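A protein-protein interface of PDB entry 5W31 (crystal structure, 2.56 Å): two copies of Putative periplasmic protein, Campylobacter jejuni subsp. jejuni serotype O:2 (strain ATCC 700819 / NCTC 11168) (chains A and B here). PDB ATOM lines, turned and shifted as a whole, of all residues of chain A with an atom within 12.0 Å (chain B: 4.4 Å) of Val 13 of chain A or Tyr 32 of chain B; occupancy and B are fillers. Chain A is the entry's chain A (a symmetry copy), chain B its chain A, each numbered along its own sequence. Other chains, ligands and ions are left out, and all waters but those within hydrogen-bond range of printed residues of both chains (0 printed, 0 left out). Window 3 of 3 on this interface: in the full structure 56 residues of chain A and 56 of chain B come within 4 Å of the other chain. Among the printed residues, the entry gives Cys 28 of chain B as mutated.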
ATOM      1  N   TYR A   4      -7.326   9.004  23.263  1.00  0.00           N
ATOM      2  CA  TYR A   4      -8.767   9.192  23.372  1.00  0.00           C
ATOM      3  C   TYR A   4      -9.198  10.438  22.617  1.00  0.00           C
ATOM      4  O   TYR A   4      -8.353  11.243  22.229  1.00  0.00           O
ATOM      5  CB  TYR A   4      -9.190   9.244  24.841  1.00  0.00           C
ATOM      6  CG  TYR A   4      -8.901   7.975  25.635  1.00  0.00           C
ATOM      7  CD1 TYR A   4      -7.559   7.585  25.966  1.00  0.00           C
ATOM      8  CD2 TYR A   4      -9.968   7.183  26.101  1.00  0.00           C
ATOM      9  CE1 TYR A   4      -7.303   6.429  26.703  1.00  0.00           C
ATOM     10  CE2 TYR A   4      -9.719   6.028  26.849  1.00  0.00           C
ATOM     11  CZ  TYR A   4      -8.399   5.651  27.145  1.00  0.00           C
ATOM     12  OH  TYR A   4      -8.216   4.501  27.888  1.00  0.00           O
ATOM     13  N   THR A   5     -10.498  10.568  22.395  1.00  0.00           N
ATOM     14  CA  THR A   5     -11.054  11.697  21.689  1.00  0.00           C
ATOM     15  C   THR A   5     -12.190  12.131  22.565  1.00  0.00           C
ATOM     16  O   THR A   5     -13.054  11.311  22.891  1.00  0.00           O
ATOM     17  CB  THR A   5     -11.596  11.295  20.275  1.00  0.00           C
ATOM     18  OG1 THR A   5     -10.507  10.903  19.431  1.00  0.00           O
ATOM     19  CG2 THR A   5     -12.377  12.457  19.579  1.00  0.00           C
ATOM     20  N   LEU A   6     -12.221  13.409  22.929  1.00  0.00           N
ATOM     21  CA  LEU A   6     -13.348  13.929  23.728  1.00  0.00           C
ATOM     22  C   LEU A   6     -14.686  13.589  23.103  1.00  0.00           C
ATOM     23  O   LEU A   6     -14.780  13.467  21.886  1.00  0.00           O
ATOM     24  CB  LEU A   6     -13.268  15.442  23.889  1.00  0.00           C
ATOM     25  CG  LEU A   6     -12.117  15.933  24.735  1.00  0.00           C
ATOM     26  CD1 LEU A   6     -11.100  16.614  23.837  1.00  0.00           C
ATOM     27  CD2 LEU A   6     -12.711  16.906  25.719  1.00  0.00           C
ATOM     28  N   ASP A   7     -15.699  13.399  23.934  1.00  0.00           N
ATOM     29  CA  ASP A   7     -17.070  13.365  23.462  1.00  0.00           C
ATOM     30  C   ASP A   7     -17.651  14.683  23.944  1.00  0.00           C
ATOM     31  O   ASP A   7     -18.180  14.780  25.057  1.00  0.00           O
ATOM     32  CB  ASP A   7     -17.828  12.108  23.959  1.00  0.00           C
ATOM     33  CG  ASP A   7     -19.379  12.248  23.905  1.00  0.00           C
ATOM     34  OD1 ASP A   7     -19.916  13.105  23.153  1.00  0.00           O
ATOM     35  OD2 ASP A   7     -20.070  11.485  24.634  1.00  0.00           O
ATOM     36  N   LYS A   8     -17.528  15.698  23.088  1.00  0.00           N
ATOM     37  CA  LYS A   8     -17.960  17.077  23.385  1.00  0.00           C
ATOM     38  C   LYS A   8     -19.386  17.163  23.959  1.00  0.00           C
ATOM     39  O   LYS A   8     -19.700  18.102  24.706  1.00  0.00           O
ATOM     40  CB  LYS A   8     -17.797  17.997  22.159  1.00  0.00           C
ATOM     41  CG  LYS A   8     -16.386  18.083  21.562  1.00  0.00           C
ATOM     42  CD  LYS A   8     -15.924  19.537  21.503  1.00  0.00           C
ATOM     43  CE  LYS A   8     -15.357  19.988  20.158  1.00  0.00           C
ATOM     44  NZ  LYS A   8     -14.019  19.405  19.883  1.00  0.00           N
ATOM     45  N   ALA A   9     -20.220  16.168  23.640  1.00  0.00           N
ATOM     46  CA  ALA A   9     -21.615  16.117  24.089  1.00  0.00           C
ATOM     47  C   ALA A   9     -21.762  15.866  25.593  1.00  0.00           C
ATOM     48  O   ALA A   9     -22.706  16.336  26.209  1.00  0.00           O
ATOM     49  CB  ALA A   9     -22.369  15.056  23.302  1.00  0.00           C
ATOM     50  N   HIS A  10     -20.833  15.105  26.172  1.00  0.00           N
ATOM     51  CA  HIS A  10     -20.866  14.751  27.603  1.00  0.00           C
ATOM     52  C   HIS A  10     -19.594  15.249  28.307  1.00  0.00           C
ATOM     53  O   HIS A  10     -19.116  14.641  29.284  1.00  0.00           O
ATOM     54  CB  HIS A  10     -21.036  13.231  27.782  1.00  0.00           C
ATOM     55  CG  HIS A  10     -22.296  12.683  27.187  1.00  0.00           C
ATOM     56  ND1 HIS A  10     -22.320  12.011  25.980  1.00  0.00           N
ATOM     57  CD2 HIS A  10     -23.575  12.709  27.631  1.00  0.00           C
ATOM     58  CE1 HIS A  10     -23.559  11.646  25.708  1.00  0.00           C
ATOM     59  NE2 HIS A  10     -24.340  12.056  26.693  1.00  0.00           N
ATOM     60  N   THR A  11     -19.042  16.335  27.761  1.00  0.00           N
ATOM     61  CA  THR A  11     -17.906  17.072  28.313  1.00  0.00           C
ATOM     62  C   THR A  11     -18.347  18.518  28.581  1.00  0.00           C
ATOM     63  O   THR A  11     -19.147  19.090  27.827  1.00  0.00           O
ATOM     64  CB  THR A  11     -16.670  16.984  27.385  1.00  0.00           C
ATOM     65  OG1 THR A  11     -16.201  15.630  27.354  1.00  0.00           O
ATOM     66  CG2 THR A  11     -15.524  17.857  27.861  1.00  0.00           C
ATOM     67  N   ASP A  12     -17.858  19.067  29.691  1.00  0.00           N
ATOM     68  CA  ASP A  12     -18.128  20.427  30.102  1.00  0.00           C
ATOM     69  C   ASP A  12     -16.774  21.046  30.544  1.00  0.00           C
ATOM     70  O   ASP A  12     -16.192  20.602  31.544  1.00  0.00           O
ATOM     71  CB  ASP A  12     -19.200  20.416  31.214  1.00  0.00           C
ATOM     72  CG  ASP A  12     -19.429  21.809  31.843  1.00  0.00           C
ATOM     73  OD1 ASP A  12     -20.247  22.586  31.296  1.00  0.00           O
ATOM     74  OD2 ASP A  12     -18.800  22.134  32.890  1.00  0.00           O
ATOM     75  N   VAL A  13     -16.259  22.021  29.778  1.00  0.00           N
ATOM     76  CA  VAL A  13     -14.999  22.701  30.116  1.00  0.00           C
ATOM     77  C   VAL A  13     -15.392  23.941  30.910  1.00  0.00           C
ATOM     78  O   VAL A  13     -15.564  25.024  30.354  1.00  0.00           O
ATOM     79  CB  VAL A  13     -14.137  22.980  28.851  1.00  0.00           C
ATOM     80  CG1 VAL A  13     -12.846  23.714  29.169  1.00  0.00           C
ATOM     81  CG2 VAL A  13     -13.788  21.671  28.154  1.00  0.00           C
ATOM     82  N   GLY A  14     -15.564  23.754  32.221  1.00  0.00           N
ATOM     83  CA  GLY A  14     -16.285  24.715  33.077  1.00  0.00           C
ATOM     84  C   GLY A  14     -15.451  25.521  34.055  1.00  0.00           C
ATOM     85  O   GLY A  14     -14.308  25.170  34.346  1.00  0.00           O
ATOM     86  N   PHE A  15     -16.042  26.605  34.565  1.00  0.00           N
ATOM     87  CA  PHE A  15     -15.412  27.501  35.552  1.00  0.00           C
ATOM     88  C   PHE A  15     -16.464  28.222  36.398  1.00  0.00           C
ATOM     89  O   PHE A  15     -17.602  28.379  35.961  1.00  0.00           O
ATOM     90  CB  PHE A  15     -14.496  28.520  34.873  1.00  0.00           C
ATOM     91  CG  PHE A  15     -15.221  29.515  34.014  1.00  0.00           C
ATOM     92  CD1 PHE A  15     -15.490  29.238  32.677  1.00  0.00           C
ATOM     93  CD2 PHE A  15     -15.634  30.742  34.539  1.00  0.00           C
ATOM     94  CE1 PHE A  15     -16.163  30.155  31.885  1.00  0.00           C
ATOM     95  CE2 PHE A  15     -16.306  31.657  33.751  1.00  0.00           C
ATOM     96  CZ  PHE A  15     -16.573  31.360  32.425  1.00  0.00           C
ATOM     97  N   LYS A  16     -16.070  28.657  37.599  1.00  0.00           N
ATOM     98  CA  LYS A  16     -16.929  29.409  38.513  1.00  0.00           C
ATOM     99  C   LYS A  16     -16.133  30.522  39.108  1.00  0.00           C
ATOM    100  O   LYS A  16     -14.976  30.328  39.529  1.00  0.00           O
ATOM    101  CB  LYS A  16     -17.476  28.550  39.653  1.00  0.00           C
ATOM    102  CG  LYS A  16     -18.803  27.894  39.345  1.00  0.00           C
ATOM    103  CD  LYS A  16     -19.324  27.118  40.549  1.00  0.00           C
ATOM    104  CE  LYS A  16     -20.438  26.132  40.172  1.00  0.00           C
ATOM    105  NZ  LYS A  16     -21.022  25.459  41.371  1.00  0.00           N
ATOM    106  N   ILE A  17     -16.751  31.693  39.142  1.00  0.00           N
ATOM    107  CA  ILE A  17     -16.108  32.863  39.739  1.00  0.00           C
ATOM    108  C   ILE A  17     -17.138  33.750  40.444  1.00  0.00           C
ATOM    109  O   ILE A  17     -18.282  33.945  39.955  1.00  0.00           O
ATOM    110  CB  ILE A  17     -15.274  33.652  38.700  1.00  0.00           C
ATOM    111  CG1 ILE A  17     -14.499  34.775  39.369  1.00  0.00           C
ATOM    112  CG2 ILE A  17     -16.137  34.121  37.516  1.00  0.00           C
ATOM    113  CD1 ILE A  17     -13.594  35.481  38.417  1.00  0.00           C
ATOM    114  N   GLY B  27     -19.778  29.138  34.027  1.00  0.00           N
ATOM    115  CA  GLY B  27     -19.434  29.286  32.626  1.00  0.00           C
ATOM    116  C   GLY B  27     -18.749  28.059  32.088  1.00  0.00           C
ATOM    117  O   GLY B  27     -18.165  27.287  32.852  1.00  0.00           O
ATOM    118  N   CYS B  28     -18.862  27.857  30.776  1.00  0.00           N
ATOM    119  CA  CYS B  28     -18.034  26.884  30.030  1.00  0.00           C
ATOM    120  C   CYS B  28     -17.585  27.480  28.717  1.00  0.00           C
ATOM    121  O   CYS B  28     -17.939  28.619  28.362  1.00  0.00           O
ATOM    122  CB  CYS B  28     -18.774  25.578  29.733  1.00  0.00           C
ATOM    123  SG  CYS B  28     -20.318  25.778  28.805  1.00  0.00           S
ATOM    124  N   PHE B  29     -16.801  26.702  27.993  1.00  0.00           N
ATOM    125  CA  PHE B  29     -16.495  27.055  26.636  1.00  0.00           C
ATOM    126  C   PHE B  29     -17.070  25.979  25.749  1.00  0.00           C
ATOM    127  O   PHE B  29     -16.792  24.778  25.953  1.00  0.00           O
ATOM    128  CB  PHE B  29     -15.009  27.201  26.459  1.00  0.00           C
ATOM    129  CG  PHE B  29     -14.419  28.297  27.281  1.00  0.00           C
ATOM    130  CD1 PHE B  29     -14.035  28.073  28.607  1.00  0.00           C
ATOM    131  CD2 PHE B  29     -14.239  29.566  26.739  1.00  0.00           C
ATOM    132  CE1 PHE B  29     -13.473  29.092  29.369  1.00  0.00           C
ATOM    133  CE2 PHE B  29     -13.680  30.584  27.507  1.00  0.00           C
ATOM    134  CZ  PHE B  29     -13.300  30.348  28.821  1.00  0.00           C
ATOM    135  N   LYS B  30     -17.906  26.421  24.801  1.00  0.00           N
ATOM    136  CA  LYS B  30     -18.633  25.531  23.906  1.00  0.00           C
ATOM    137  C   LYS B  30     -17.683  24.888  22.849  1.00  0.00           C
ATOM    138  O   LYS B  30     -17.943  23.773  22.390  1.00  0.00           O
ATOM    139  CB  LYS B  30     -19.875  26.232  23.321  1.00  0.00           C
ATOM    140  N   ASP B  31     -16.551  25.533  22.542  1.00  0.00           N
ATOM    141  CA  ASP B  31     -15.629  25.023  21.518  1.00  0.00           C
ATOM    142  C   ASP B  31     -14.117  25.006  21.858  1.00  0.00           C
ATOM    143  O   ASP B  31     -13.506  26.049  22.127  1.00  0.00           O
ATOM    144  CB  ASP B  31     -15.876  25.783  20.206  1.00  0.00           C
ATOM    145  CG  ASP B  31     -15.045  25.262  19.062  1.00  0.00           C
ATOM    146  OD1 ASP B  31     -14.972  24.013  18.878  1.00  0.00           O
ATOM    147  OD2 ASP B  31     -14.470  26.122  18.360  1.00  0.00           O
ATOM    148  N   TYR B  32     -13.527  23.816  21.769  1.00  0.00           N
ATOM    149  CA  TYR B  32     -12.183  23.508  22.285  1.00  0.00           C
ATOM    150  C   TYR B  32     -11.733  22.220  21.611  1.00  0.00           C
ATOM    151  O   TYR B  32     -12.565  21.441  21.135  1.00  0.00           O
ATOM    152  CB  TYR B  32     -12.227  23.244  23.820  1.00  0.00           C
ATOM    153  CG  TYR B  32     -13.323  22.237  24.244  1.00  0.00           C
ATOM    154  CD1 TYR B  32     -14.648  22.659  24.408  1.00  0.00           C
ATOM    155  CD2 TYR B  32     -13.043  20.875  24.445  1.00  0.00           C
ATOM    156  CE1 TYR B  32     -15.664  21.777  24.750  1.00  0.00           C
ATOM    157  CE2 TYR B  32     -14.063  19.979  24.784  1.00  0.00           C
ATOM    158  CZ  TYR B  32     -15.376  20.441  24.935  1.00  0.00           C
ATOM    159  OH  TYR B  32     -16.437  19.616  25.273  1.00  0.00           O
ATOM    160  N   SER B  33     -10.434  21.973  21.584  1.00  0.00           N
ATOM    161  CA  SER B  33      -9.933  20.659  21.190  1.00  0.00           C
ATOM    162  C   SER B  33      -8.988  20.107  22.267  1.00  0.00           C
ATOM    163  O   SER B  33      -8.417  20.871  23.065  1.00  0.00           O
ATOM    164  CB  SER B  33      -9.203  20.742  19.844  1.00  0.00           C
ATOM    165  OG  SER B  33      -7.803  20.935  20.024  1.00  0.00           O
ATOM    166  N   THR B  51      -6.804  23.166  23.847  1.00  0.00           N
ATOM    167  CA  THR B  51      -6.894  24.505  23.250  1.00  0.00           C
ATOM    168  C   THR B  51      -8.349  24.882  23.283  1.00  0.00           C
ATOM    169  O   THR B  51      -9.206  24.098  22.848  1.00  0.00           O
ATOM    170  CB  THR B  51      -6.380  24.539  21.791  1.00  0.00           C
ATOM    171  OG1 THR B  51      -4.959  24.461  21.809  1.00  0.00           O
ATOM    172  CG2 THR B  51      -6.736  25.838  21.084  1.00  0.00           C
ATOM    173  N   ILE B  52      -8.618  26.084  23.788  1.00  0.00           N
ATOM    174  CA  ILE B  52      -9.981  26.543  23.997  1.00  0.00           C
ATOM    175  C   ILE B  52     -10.172  27.819  23.219  1.00  0.00           C
ATOM    176  O   ILE B  52      -9.335  28.730  23.332  1.00  0.00           O
ATOM    177  CB  ILE B  52     -10.225  26.839  25.482  1.00  0.00           C
ATOM    178  CG1 ILE B  52     -10.178  25.554  26.294  1.00  0.00           C
ATOM    179  CG2 ILE B  52     -11.588  27.468  25.680  1.00  0.00           C
ATOM    180  CD1 ILE B  52      -9.664  25.799  27.685  1.00  0.00           C
ATOM    181  N   ASN B 162     -13.570  23.616  36.736  1.00  0.00           N
ATOM    182  CA  ASN B 162     -14.163  22.303  36.780  1.00  0.00           C
ATOM    183  C   ASN B 162     -14.256  21.707  35.339  1.00  0.00           C
ATOM    184  O   ASN B 162     -15.170  22.047  34.564  1.00  0.00           O
ATOM    185  CB  ASN B 162     -15.507  22.332  37.537  1.00  0.00           C
ATOM    186  CG  ASN B 162     -16.238  20.998  37.451  1.00  0.00           C
ATOM    187  OD1 ASN B 162     -17.079  20.799  36.572  1.00  0.00           O
ATOM    188  ND2 ASN B 162     -15.861  20.047  38.305  1.00  0.00           N
ATOM    189  N   ILE B 163     -13.296  20.850  34.981  1.00  0.00           N
ATOM    190  CA  ILE B 163     -13.295  20.204  33.670  1.00  0.00           C
ATOM    191  C   ILE B 163     -13.858  18.809  33.850  1.00  0.00           C
ATOM    192  O   ILE B 163     -13.275  17.987  34.558  1.00  0.00           O
ATOM    193  CB  ILE B 163     -11.880  20.082  33.054  1.00  0.00           C
ATOM    194  CG1 ILE B 163     -11.033  21.347  33.255  1.00  0.00           C
ATOM    195  CG2 ILE B 163     -11.948  19.698  31.589  1.00  0.00           C
ATOM    196  CD1 ILE B 163     -11.726  22.657  32.978  1.00  0.00           C
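N of Phe 15 of chain A is in hydrogen-bond range of O of Gly 27 of chain B. O of Val 13 of chain A sits at hydrogen-bond distance from N of Phe 29 of chain B (3.1 Å). O of Tyr 32 of chain B sits at hydrogen-bond distance from NZ of Lys 8 of chain A, at 2.8 Å. The backbone carbonyl oxygen (O) of Asn 162 of chain B is in hydrogen-bond range of the backbone NH (N) of Gly 14 of chain A (2.9 Å).
Hydrophobic or aromatic side chains of chain A that line the printed part of chain B: Leu 6, Val 13 and Phe 15. Hydrophobic or aromatic side chains of chain B within 4 Å of the printed part of chain A: Phe 29, Tyr 32 and Ile 163. Among the printed residues, no Asp or Glu carboxylate lies within 4 Å of a Lys or Arg side-chain nitrogen of the other chain.
The backbone carbonyl oxygen (O) of Asp 7 of chain A sits at hydrogen-bond distance from the side-chain hydroxyl (OG1) of Thr 11 of chain A (3.1 Å).
CE2 of Tyr 32 of chain B touches CD2 of Leu 6 of chain A, 3.5 Å away. Thr 11 of chain A touches Tyr 32 of chain B (CG2 to OH, 3.3 Å). Cys 28 of chain B touches Asp 12 of chain A (CB to OD1, 3.7 Å). Asp 12 of chain A touches Asn 162 of chain B. Asp 12 of chain A touches Ile 163 of chain B. O of Val 13 of chain A touches CA of Cys 28 of chain B, at 3.1 Å. CE2 of Tyr 32 of chain B touches CG2 of Val 13 of chain A, 3.8 Å away. O of Gly 27 of chain B touches CA of Gly 14 of chain A, at 3.2 Å. Ile 163 of chain B touches Gly 14 of chain A (CD1 to O, 3.9 Å). Phe 29 of chain B touches Phe 15 of chain A (CE1 to CE1, 3.8 Å).
No position is printed for both chains. Of the 15 pairs that touch across the chains among the printed residues, none has its exchanged pair printed and touching as well.
Val 13 of chain A touches just these residues of chain B: Cys 28 (3.1 Å), Phe 29 (3.1 Å) and Tyr 32 (3.8 Å). Tyr 32 of chain B touches just these residues of chain A: Leu 6, Lys 8, Thr 11 and Val 13. Gly 27 of chain B touches two residues of chain A. Cys 28 of chain B touches just these residues of chain A: Asp 12, Val 13 and Phe 15. Of chain A, only Val 13 and Phe 15 come within 4 Å of Phe 29 of chain B. No residue of chain A comes within 4 Å of Lys 30 of chain B. No residue of chain A comes within 4 Å of Ser 33 of chain B. Thr 51 of chain B touches none of the printed residues of chain A. Of the printed residues of chain B, Asp 12 of chain A touches Cys 28 (3.7 Å), Asn 162 (3.5 Å) and Ile 163 (3.6 Å). Printed residues of chain B within 4 Å of Leu 6 of chain A: Tyr 32. Lys 16 of chain A touches none of the printed residues of chain B. Thr 5 of chain A touches none of the printed residues of chain B.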
